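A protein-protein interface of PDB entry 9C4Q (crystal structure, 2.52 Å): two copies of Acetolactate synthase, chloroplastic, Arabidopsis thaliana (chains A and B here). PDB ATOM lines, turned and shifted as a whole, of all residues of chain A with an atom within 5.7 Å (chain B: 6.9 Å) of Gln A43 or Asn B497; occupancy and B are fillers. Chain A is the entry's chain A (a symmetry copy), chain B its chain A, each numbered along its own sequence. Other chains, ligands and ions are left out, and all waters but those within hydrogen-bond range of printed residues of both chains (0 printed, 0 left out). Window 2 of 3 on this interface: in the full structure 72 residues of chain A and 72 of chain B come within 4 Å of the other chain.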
ATOM      1  N   ASP A  16     -19.669  12.928  25.715  1.00  0.00           N
ATOM      2  CA  ASP A  16     -18.729  11.813  25.735  1.00  0.00           C
ATOM      3  C   ASP A  16     -19.435  10.481  25.527  1.00  0.00           C
ATOM      4  O   ASP A  16     -18.859   9.559  24.935  1.00  0.00           O
ATOM      5  CB  ASP A  16     -17.955  11.812  27.051  1.00  0.00           C
ATOM      6  CG  ASP A  16     -16.978  12.965  27.147  1.00  0.00           C
ATOM      7  OD1 ASP A  16     -16.072  13.048  26.291  1.00  0.00           O
ATOM      8  OD2 ASP A  16     -17.121  13.793  28.071  1.00  0.00           O
ATOM      9  N   SER A  38     -23.091  22.730  19.529  1.00  0.00           N
ATOM     10  CA  SER A  38     -22.388  21.458  19.411  1.00  0.00           C
ATOM     11  C   SER A  38     -20.957  21.524  19.932  1.00  0.00           C
ATOM     12  O   SER A  38     -20.167  20.612  19.651  1.00  0.00           O
ATOM     13  CB  SER A  38     -22.388  20.977  17.956  1.00  0.00           C
ATOM     14  OG  SER A  38     -21.637  21.850  17.127  1.00  0.00           O
ATOM     15  N   MET A  39     -20.600  22.572  20.683  1.00  0.00           N
ATOM     16  CA  MET A  39     -19.233  22.688  21.187  1.00  0.00           C
ATOM     17  C   MET A  39     -18.863  21.504  22.071  1.00  0.00           C
ATOM     18  O   MET A  39     -17.729  21.014  22.022  1.00  0.00           O
ATOM     19  CB  MET A  39     -19.053  23.992  21.964  1.00  0.00           C
ATOM     20  CG  MET A  39     -19.008  25.249  21.116  1.00  0.00           C
ATOM     21  SD  MET A  39     -18.450  26.675  22.068  1.00  0.00           S
ATOM     22  CE  MET A  39     -16.787  26.161  22.488  1.00  0.00           C
ATOM     23  N   GLU A  40     -19.807  21.035  22.893  1.00  0.00           N
ATOM     24  CA  GLU A  40     -19.527  19.907  23.775  1.00  0.00           C
ATOM     25  C   GLU A  40     -19.181  18.655  22.980  1.00  0.00           C
ATOM     26  O   GLU A  40     -18.274  17.902  23.356  1.00  0.00           O
ATOM     27  CB  GLU A  40     -20.724  19.649  24.690  1.00  0.00           C
ATOM     28  CG  GLU A  40     -20.960  20.734  25.729  1.00  0.00           C
ATOM     29  CD  GLU A  40     -19.947  20.693  26.855  1.00  0.00           C
ATOM     30  OE1 GLU A  40     -19.302  19.640  27.040  1.00  0.00           O
ATOM     31  OE2 GLU A  40     -19.798  21.715  27.556  1.00  0.00           O
ATOM     32  N   ILE A  41     -19.892  18.418  21.875  1.00  0.00           N
ATOM     33  CA  ILE A  41     -19.596  17.268  21.025  1.00  0.00           C
ATOM     34  C   ILE A  41     -18.197  17.387  20.437  1.00  0.00           C
ATOM     35  O   ILE A  41     -17.450  16.403  20.365  1.00  0.00           O
ATOM     36  CB  ILE A  41     -20.665  17.134  19.925  1.00  0.00           C
ATOM     37  CG1 ILE A  41     -22.028  16.819  20.544  1.00  0.00           C
ATOM     38  CG2 ILE A  41     -20.269  16.072  18.908  1.00  0.00           C
ATOM     39  CD1 ILE A  41     -23.169  16.877  19.554  1.00  0.00           C
ATOM     40  N   HIS A  42     -17.813  18.594  20.017  1.00  0.00           N
ATOM     41  CA  HIS A  42     -16.495  18.780  19.419  1.00  0.00           C
ATOM     42  C   HIS A  42     -15.388  18.624  20.453  1.00  0.00           C
ATOM     43  O   HIS A  42     -14.312  18.102  20.139  1.00  0.00           O
ATOM     44  CB  HIS A  42     -16.414  20.142  18.731  1.00  0.00           C
ATOM     45  CG  HIS A  42     -17.027  20.157  17.368  1.00  0.00           C
ATOM     46  ND1 HIS A  42     -16.282  20.011  16.219  1.00  0.00           N
ATOM     47  CD2 HIS A  42     -18.314  20.286  16.970  1.00  0.00           C
ATOM     48  CE1 HIS A  42     -17.083  20.056  15.170  1.00  0.00           C
ATOM     49  NE2 HIS A  42     -18.322  20.219  15.598  1.00  0.00           N
ATOM     50  N   GLN A  43     -15.623  19.076  21.686  1.00  0.00           N
ATOM     51  CA  GLN A  43     -14.654  18.836  22.751  1.00  0.00           C
ATOM     52  C   GLN A  43     -14.485  17.344  22.999  1.00  0.00           C
ATOM     53  O   GLN A  43     -13.364  16.850  23.158  1.00  0.00           O
ATOM     54  CB  GLN A  43     -15.089  19.543  24.034  1.00  0.00           C
ATOM     55  CG  GLN A  43     -14.998  21.057  23.977  1.00  0.00           C
ATOM     56  CD  GLN A  43     -13.566  21.552  23.962  1.00  0.00           C
ATOM     57  OE1 GLN A  43     -12.714  21.044  24.691  1.00  0.00           O
ATOM     58  NE2 GLN A  43     -13.292  22.546  23.127  1.00  0.00           N
ATOM     59  N   ALA A  44     -15.599  16.608  23.022  1.00  0.00           N
ATOM     60  CA  ALA A  44     -15.539  15.166  23.227  1.00  0.00           C
ATOM     61  C   ALA A  44     -14.847  14.463  22.067  1.00  0.00           C
ATOM     62  O   ALA A  44     -14.247  13.400  22.263  1.00  0.00           O
ATOM     63  CB  ALA A  44     -16.949  14.607  23.427  1.00  0.00           C
ATOM     64  N   LEU A  45     -14.913  15.037  20.863  1.00  0.00           N
ATOM     65  CA  LEU A  45     -14.233  14.430  19.722  1.00  0.00           C
ATOM     66  C   LEU A  45     -12.720  14.480  19.885  1.00  0.00           C
ATOM     67  O   LEU A  45     -12.025  13.513  19.555  1.00  0.00           O
ATOM     68  CB  LEU A  45     -14.659  15.124  18.426  1.00  0.00           C
ATOM     69  CG  LEU A  45     -16.027  14.744  17.858  1.00  0.00           C
ATOM     70  CD1 LEU A  45     -16.335  15.555  16.608  1.00  0.00           C
ATOM     71  CD2 LEU A  45     -16.086  13.253  17.557  1.00  0.00           C
ATOM     72  N   THR A  46     -12.192  15.597  20.395  1.00  0.00           N
ATOM     73  CA  THR A  46     -10.755  15.701  20.618  1.00  0.00           C
ATOM     74  C   THR A  46     -10.266  14.702  21.657  1.00  0.00           C
ATOM     75  O   THR A  46      -9.077  14.362  21.665  1.00  0.00           O
ATOM     76  CB  THR A  46     -10.384  17.123  21.045  1.00  0.00           C
ATOM     77  OG1 THR A  46     -10.923  17.389  22.347  1.00  0.00           O
ATOM     78  CG2 THR A  46     -10.945  18.134  20.060  1.00  0.00           C
ATOM     79  N   ARG A  47     -11.151  14.223  22.532  1.00  0.00           N
ATOM     80  CA  ARG A  47     -10.795  13.199  23.504  1.00  0.00           C
ATOM     81  C   ARG A  47     -10.786  11.798  22.911  1.00  0.00           C
ATOM     82  O   ARG A  47     -10.279  10.876  23.557  1.00  0.00           O
ATOM     83  CB  ARG A  47     -11.758  13.245  24.695  1.00  0.00           C
ATOM     84  CG  ARG A  47     -11.743  14.566  25.443  1.00  0.00           C
ATOM     85  CD  ARG A  47     -12.720  14.570  26.606  1.00  0.00           C
ATOM     86  NE  ARG A  47     -13.085  15.934  26.976  1.00  0.00           N
ATOM     87  CZ  ARG A  47     -14.310  16.435  26.895  1.00  0.00           C
ATOM     88  NH1 ARG A  47     -15.338  15.694  26.521  1.00  0.00           N
ATOM     89  NH2 ARG A  47     -14.510  17.714  27.203  1.00  0.00           N
ATOM     90  N   GLU B 490     -14.067  28.686  23.651  1.00  0.00           N
ATOM     91  CA  GLU B 490     -13.071  27.699  24.055  1.00  0.00           C
ATOM     92  C   GLU B 490     -12.127  28.280  25.103  1.00  0.00           C
ATOM     93  O   GLU B 490     -11.813  27.625  26.102  1.00  0.00           O
ATOM     94  CB  GLU B 490     -12.289  27.209  22.834  1.00  0.00           C
ATOM     95  CG  GLU B 490     -13.114  26.389  21.849  1.00  0.00           C
ATOM     96  CD  GLU B 490     -12.329  25.985  20.616  1.00  0.00           C
ATOM     97  OE1 GLU B 490     -11.457  26.764  20.181  1.00  0.00           O
ATOM     98  OE2 GLU B 490     -12.587  24.888  20.081  1.00  0.00           O
ATOM     99  N   ASP B 491     -11.680  29.522  24.896  1.00  0.00           N
ATOM    100  CA  ASP B 491     -10.776  30.158  25.852  1.00  0.00           C
ATOM    101  C   ASP B 491     -11.439  30.329  27.214  1.00  0.00           C
ATOM    102  O   ASP B 491     -10.836  30.034  28.252  1.00  0.00           O
ATOM    103  CB  ASP B 491     -10.315  31.515  25.315  1.00  0.00           C
ATOM    104  CG  ASP B 491      -9.466  31.394  24.067  1.00  0.00           C
ATOM    105  OD1 ASP B 491      -8.940  30.291  23.813  1.00  0.00           O
ATOM    106  OD2 ASP B 491      -9.318  32.405  23.347  1.00  0.00           O
ATOM    107  N   TYR B 494     -13.497  26.301  28.097  1.00  0.00           N
ATOM    108  CA  TYR B 494     -12.928  24.990  27.805  1.00  0.00           C
ATOM    109  C   TYR B 494     -11.404  25.018  27.831  1.00  0.00           C
ATOM    110  O   TYR B 494     -10.754  24.228  27.137  1.00  0.00           O
ATOM    111  CB  TYR B 494     -13.439  24.464  26.464  1.00  0.00           C
ATOM    112  CG  TYR B 494     -14.942  24.313  26.425  1.00  0.00           C
ATOM    113  CD1 TYR B 494     -15.561  23.184  26.943  1.00  0.00           C
ATOM    114  CD2 TYR B 494     -15.746  25.305  25.876  1.00  0.00           C
ATOM    115  CE1 TYR B 494     -16.937  23.044  26.914  1.00  0.00           C
ATOM    116  CE2 TYR B 494     -17.122  25.174  25.843  1.00  0.00           C
ATOM    117  CZ  TYR B 494     -17.712  24.043  26.361  1.00  0.00           C
ATOM    118  OH  TYR B 494     -19.081  23.910  26.326  1.00  0.00           O
ATOM    119  N   LYS B 495     -10.824  25.921  28.628  1.00  0.00           N
ATOM    120  CA  LYS B 495      -9.382  25.951  28.882  1.00  0.00           C
ATOM    121  C   LYS B 495      -8.582  26.080  27.586  1.00  0.00           C
ATOM    122  O   LYS B 495      -7.493  25.516  27.449  1.00  0.00           O
ATOM    123  CB  LYS B 495      -8.940  24.719  29.677  1.00  0.00           C
ATOM    124  CG  LYS B 495      -9.484  24.683  31.097  1.00  0.00           C
ATOM    125  CD  LYS B 495      -9.240  23.335  31.757  1.00  0.00           C
ATOM    126  CE  LYS B 495      -9.406  23.416  33.267  1.00  0.00           C
ATOM    127  NZ  LYS B 495     -10.699  24.039  33.665  1.00  0.00           N
ATOM    128  N   ALA B 496      -9.135  26.827  26.627  1.00  0.00           N
ATOM    129  CA  ALA B 496      -8.469  27.109  25.354  1.00  0.00           C
ATOM    130  C   ALA B 496      -8.152  25.833  24.579  1.00  0.00           C
ATOM    131  O   ALA B 496      -7.200  25.787  23.798  1.00  0.00           O
ATOM    132  CB  ALA B 496      -7.200  27.940  25.565  1.00  0.00           C
ATOM    133  N   ASN B 497      -8.946  24.785  24.782  1.00  0.00           N
ATOM    134  CA  ASN B 497      -8.745  23.532  24.064  1.00  0.00           C
ATOM    135  C   ASN B 497      -9.390  23.651  22.689  1.00  0.00           C
ATOM    136  O   ASN B 497     -10.619  23.677  22.568  1.00  0.00           O
ATOM    137  CB  ASN B 497      -9.317  22.359  24.853  1.00  0.00           C
ATOM    138  CG  ASN B 497      -9.085  21.027  24.165  1.00  0.00           C
ATOM    139  OD1 ASN B 497      -7.945  20.610  23.961  1.00  0.00           O
ATOM    140  ND2 ASN B 497     -10.171  20.349  23.812  1.00  0.00           N
ATOM    141  N   ARG B 498      -8.556  23.734  21.654  1.00  0.00           N
ATOM    142  CA  ARG B 498      -9.042  23.945  20.298  1.00  0.00           C
ATOM    143  C   ARG B 498      -9.713  22.686  19.767  1.00  0.00           C
ATOM    144  O   ARG B 498      -9.127  21.600  19.784  1.00  0.00           O
ATOM    145  CB  ARG B 498      -7.887  24.350  19.384  1.00  0.00           C
ATOM    146  CG  ARG B 498      -7.238  25.672  19.750  1.00  0.00           C
ATOM    147  CD  ARG B 498      -8.086  26.851  19.296  1.00  0.00           C
ATOM    148  NE  ARG B 498      -7.568  28.114  19.808  1.00  0.00           N
ATOM    149  CZ  ARG B 498      -8.005  28.712  20.908  1.00  0.00           C
ATOM    150  NH1 ARG B 498      -8.987  28.197  21.629  1.00  0.00           N
ATOM    151  NH2 ARG B 498      -7.449  29.857  21.286  1.00  0.00           N
ATOM    152  N   ALA B 499     -10.954  22.834  19.300  1.00  0.00           N
ATOM    153  CA  ALA B 499     -11.725  21.739  18.720  1.00  0.00           C
ATOM    154  C   ALA B 499     -12.224  22.181  17.339  1.00  0.00           C
ATOM    155  O   ALA B 499     -13.401  22.504  17.162  1.00  0.00           O
ATOM    156  CB  ALA B 499     -12.874  21.321  19.639  1.00  0.00           C
ATOM    157  N   HIS B 500     -11.302  22.214  16.371  1.00  0.00           N
ATOM    158  CA  HIS B 500     -11.598  22.433  14.956  1.00  0.00           C
ATOM    159  C   HIS B 500     -12.034  23.864  14.658  1.00  0.00           C
ATOM    160  O   HIS B 500     -12.880  24.092  13.788  1.00  0.00           O
ATOM    161  CB  HIS B 500     -12.662  21.447  14.470  1.00  0.00           C
ATOM    162  CG  HIS B 500     -12.497  20.062  15.015  1.00  0.00           C
ATOM    163  ND1 HIS B 500     -13.341  19.532  15.968  1.00  0.00           N
ATOM    164  CD2 HIS B 500     -11.568  19.110  14.762  1.00  0.00           C
ATOM    165  CE1 HIS B 500     -12.945  18.309  16.270  1.00  0.00           C
ATOM    166  NE2 HIS B 500     -11.873  18.028  15.551  1.00  0.00           N
ATOM    167  N   THR B 501     -11.444  24.837  15.354  1.00  0.00           N
ATOM    168  CA  THR B 501     -11.739  26.243  15.118  1.00  0.00           C
ATOM    169  C   THR B 501     -10.675  26.953  14.290  1.00  0.00           C
ATOM    170  O   THR B 501     -10.876  28.113  13.922  1.00  0.00           O
ATOM    171  CB  THR B 501     -11.912  26.984  16.449  1.00  0.00           C
ATOM    172  OG1 THR B 501     -10.815  26.673  17.317  1.00  0.00           O
ATOM    173  CG2 THR B 501     -13.219  26.589  17.115  1.00  0.00           C
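Asp A16 touches none of the printed residues of chain B.
Of the printed residues of chain B, Glu A40 touches Tyr B494.
Printed residues of chain B within 4 Å of His A42: Ala B499 (3.6 Å) and His B500 (3.0 Å).
Of the printed residues of chain B, Gln A43 touches Glu B490, Tyr B494, Asn B497 and Ala B499.
Printed residues of chain A within 4 Å of Glu B490: Met A39 and Gln A43.
Asn B497 touches just these residues of chain A: Gln A43 (2.8 Å) and Thr A46 (3.4 Å).
Of the printed residues of chain A, Ala B499 touches His A42 (3.6 Å), Gln A43 (3.7 Å) and Thr A46 (3.7 Å).
Thr B501 touches none of the printed residues of chain A.
The nearest residue of chain B that does not touch Gln A43 is Arg B498 (4.9 Å).
The nearest printed residue of chain A that does not touch Asn B497 is His A42 (6.0 Å).
The nearest printed residue of chain B that does not touch His A42 is Asn B497 (6.0 Å).
Of the 10 printed residues of chain B, 6 touch a printed residue of chain A.
Hydrophobic or aromatic side chains of chain B that line the printed part of chain A: Tyr B494, Ala B499 and His B500.
Of the 11 printed residues of chain A, 5 touch a printed residue of chain B.
Hydrophobic or aromatic side chains of chain A that line the printed part of chain B: Met A39 and His A42.
Among the printed residues, 12 pairs touch across the chains.
The backbone carbonyl oxygen (O) of Glu B490 lies within hydrogen-bond range of the backbone NH (N) of Ala B496 (2.8 Å).
The side-chain carboxylate (OE1) of Glu B490 lies within salt-bridge range of the guanidinium group (NH1) of Arg B498, 3.2 Å away.
The backbone NH (N) of Ala B499 is in hydrogen-bond range of the side-chain carboxylate (OE2) of Glu B490, 2.7 Å away.
OE1 of Glu B490 is in hydrogen-bond range of OG1 of Thr B501 (2.9 Å).
OD1 of Asp B491 lies within salt-bridge range of NH2 of Arg B498 (3.0 Å).
The backbone carbonyl oxygen (O) of Gln A43 sits at hydrogen-bond distance from the side-chain hydroxyl (OG1) of Thr A46 (2.6 Å).
OH of Tyr B494 sits at hydrogen-bond distance from OE2 of Glu A40 (2.6 Å).
The side-chain amide oxygen of Gln A43 is in hydrogen-bond range of the side-chain amide nitrogen of Asn B497.
The side-chain hydroxyl of Thr A46 is in hydrogen-bond range of the side-chain amide nitrogen of Asn B497, 3.4 Å away.
ND1 of His B500 sits at hydrogen-bond distance from ND1 of His A42 (3.0 Å).
Met A39 touches Glu B490.
Met A39 touches Tyr B494 (CE to CE2, 3.5 Å).
O of His A42 touches CB of Ala B499, 3.6 Å away.
OE2 of Glu B490 touches NE2 of Gln A43 (3.9 Å).
CD1 of Tyr B494 touches CG of Gln A43, at 3.7 Å.
Ala B499 touches Gln A43 (CB to NE2, 3.7 Å).
Thr A46 touches Arg B498 (CG2 to O, 3.9 Å).
Thr A46 touches Ala B499 (CG2 to CB, 3.7 Å).
No position is printed for both chains.
Of the 12 pairs that touch across the chains among the printed residues, none has its exchanged pair printed and touching as well.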
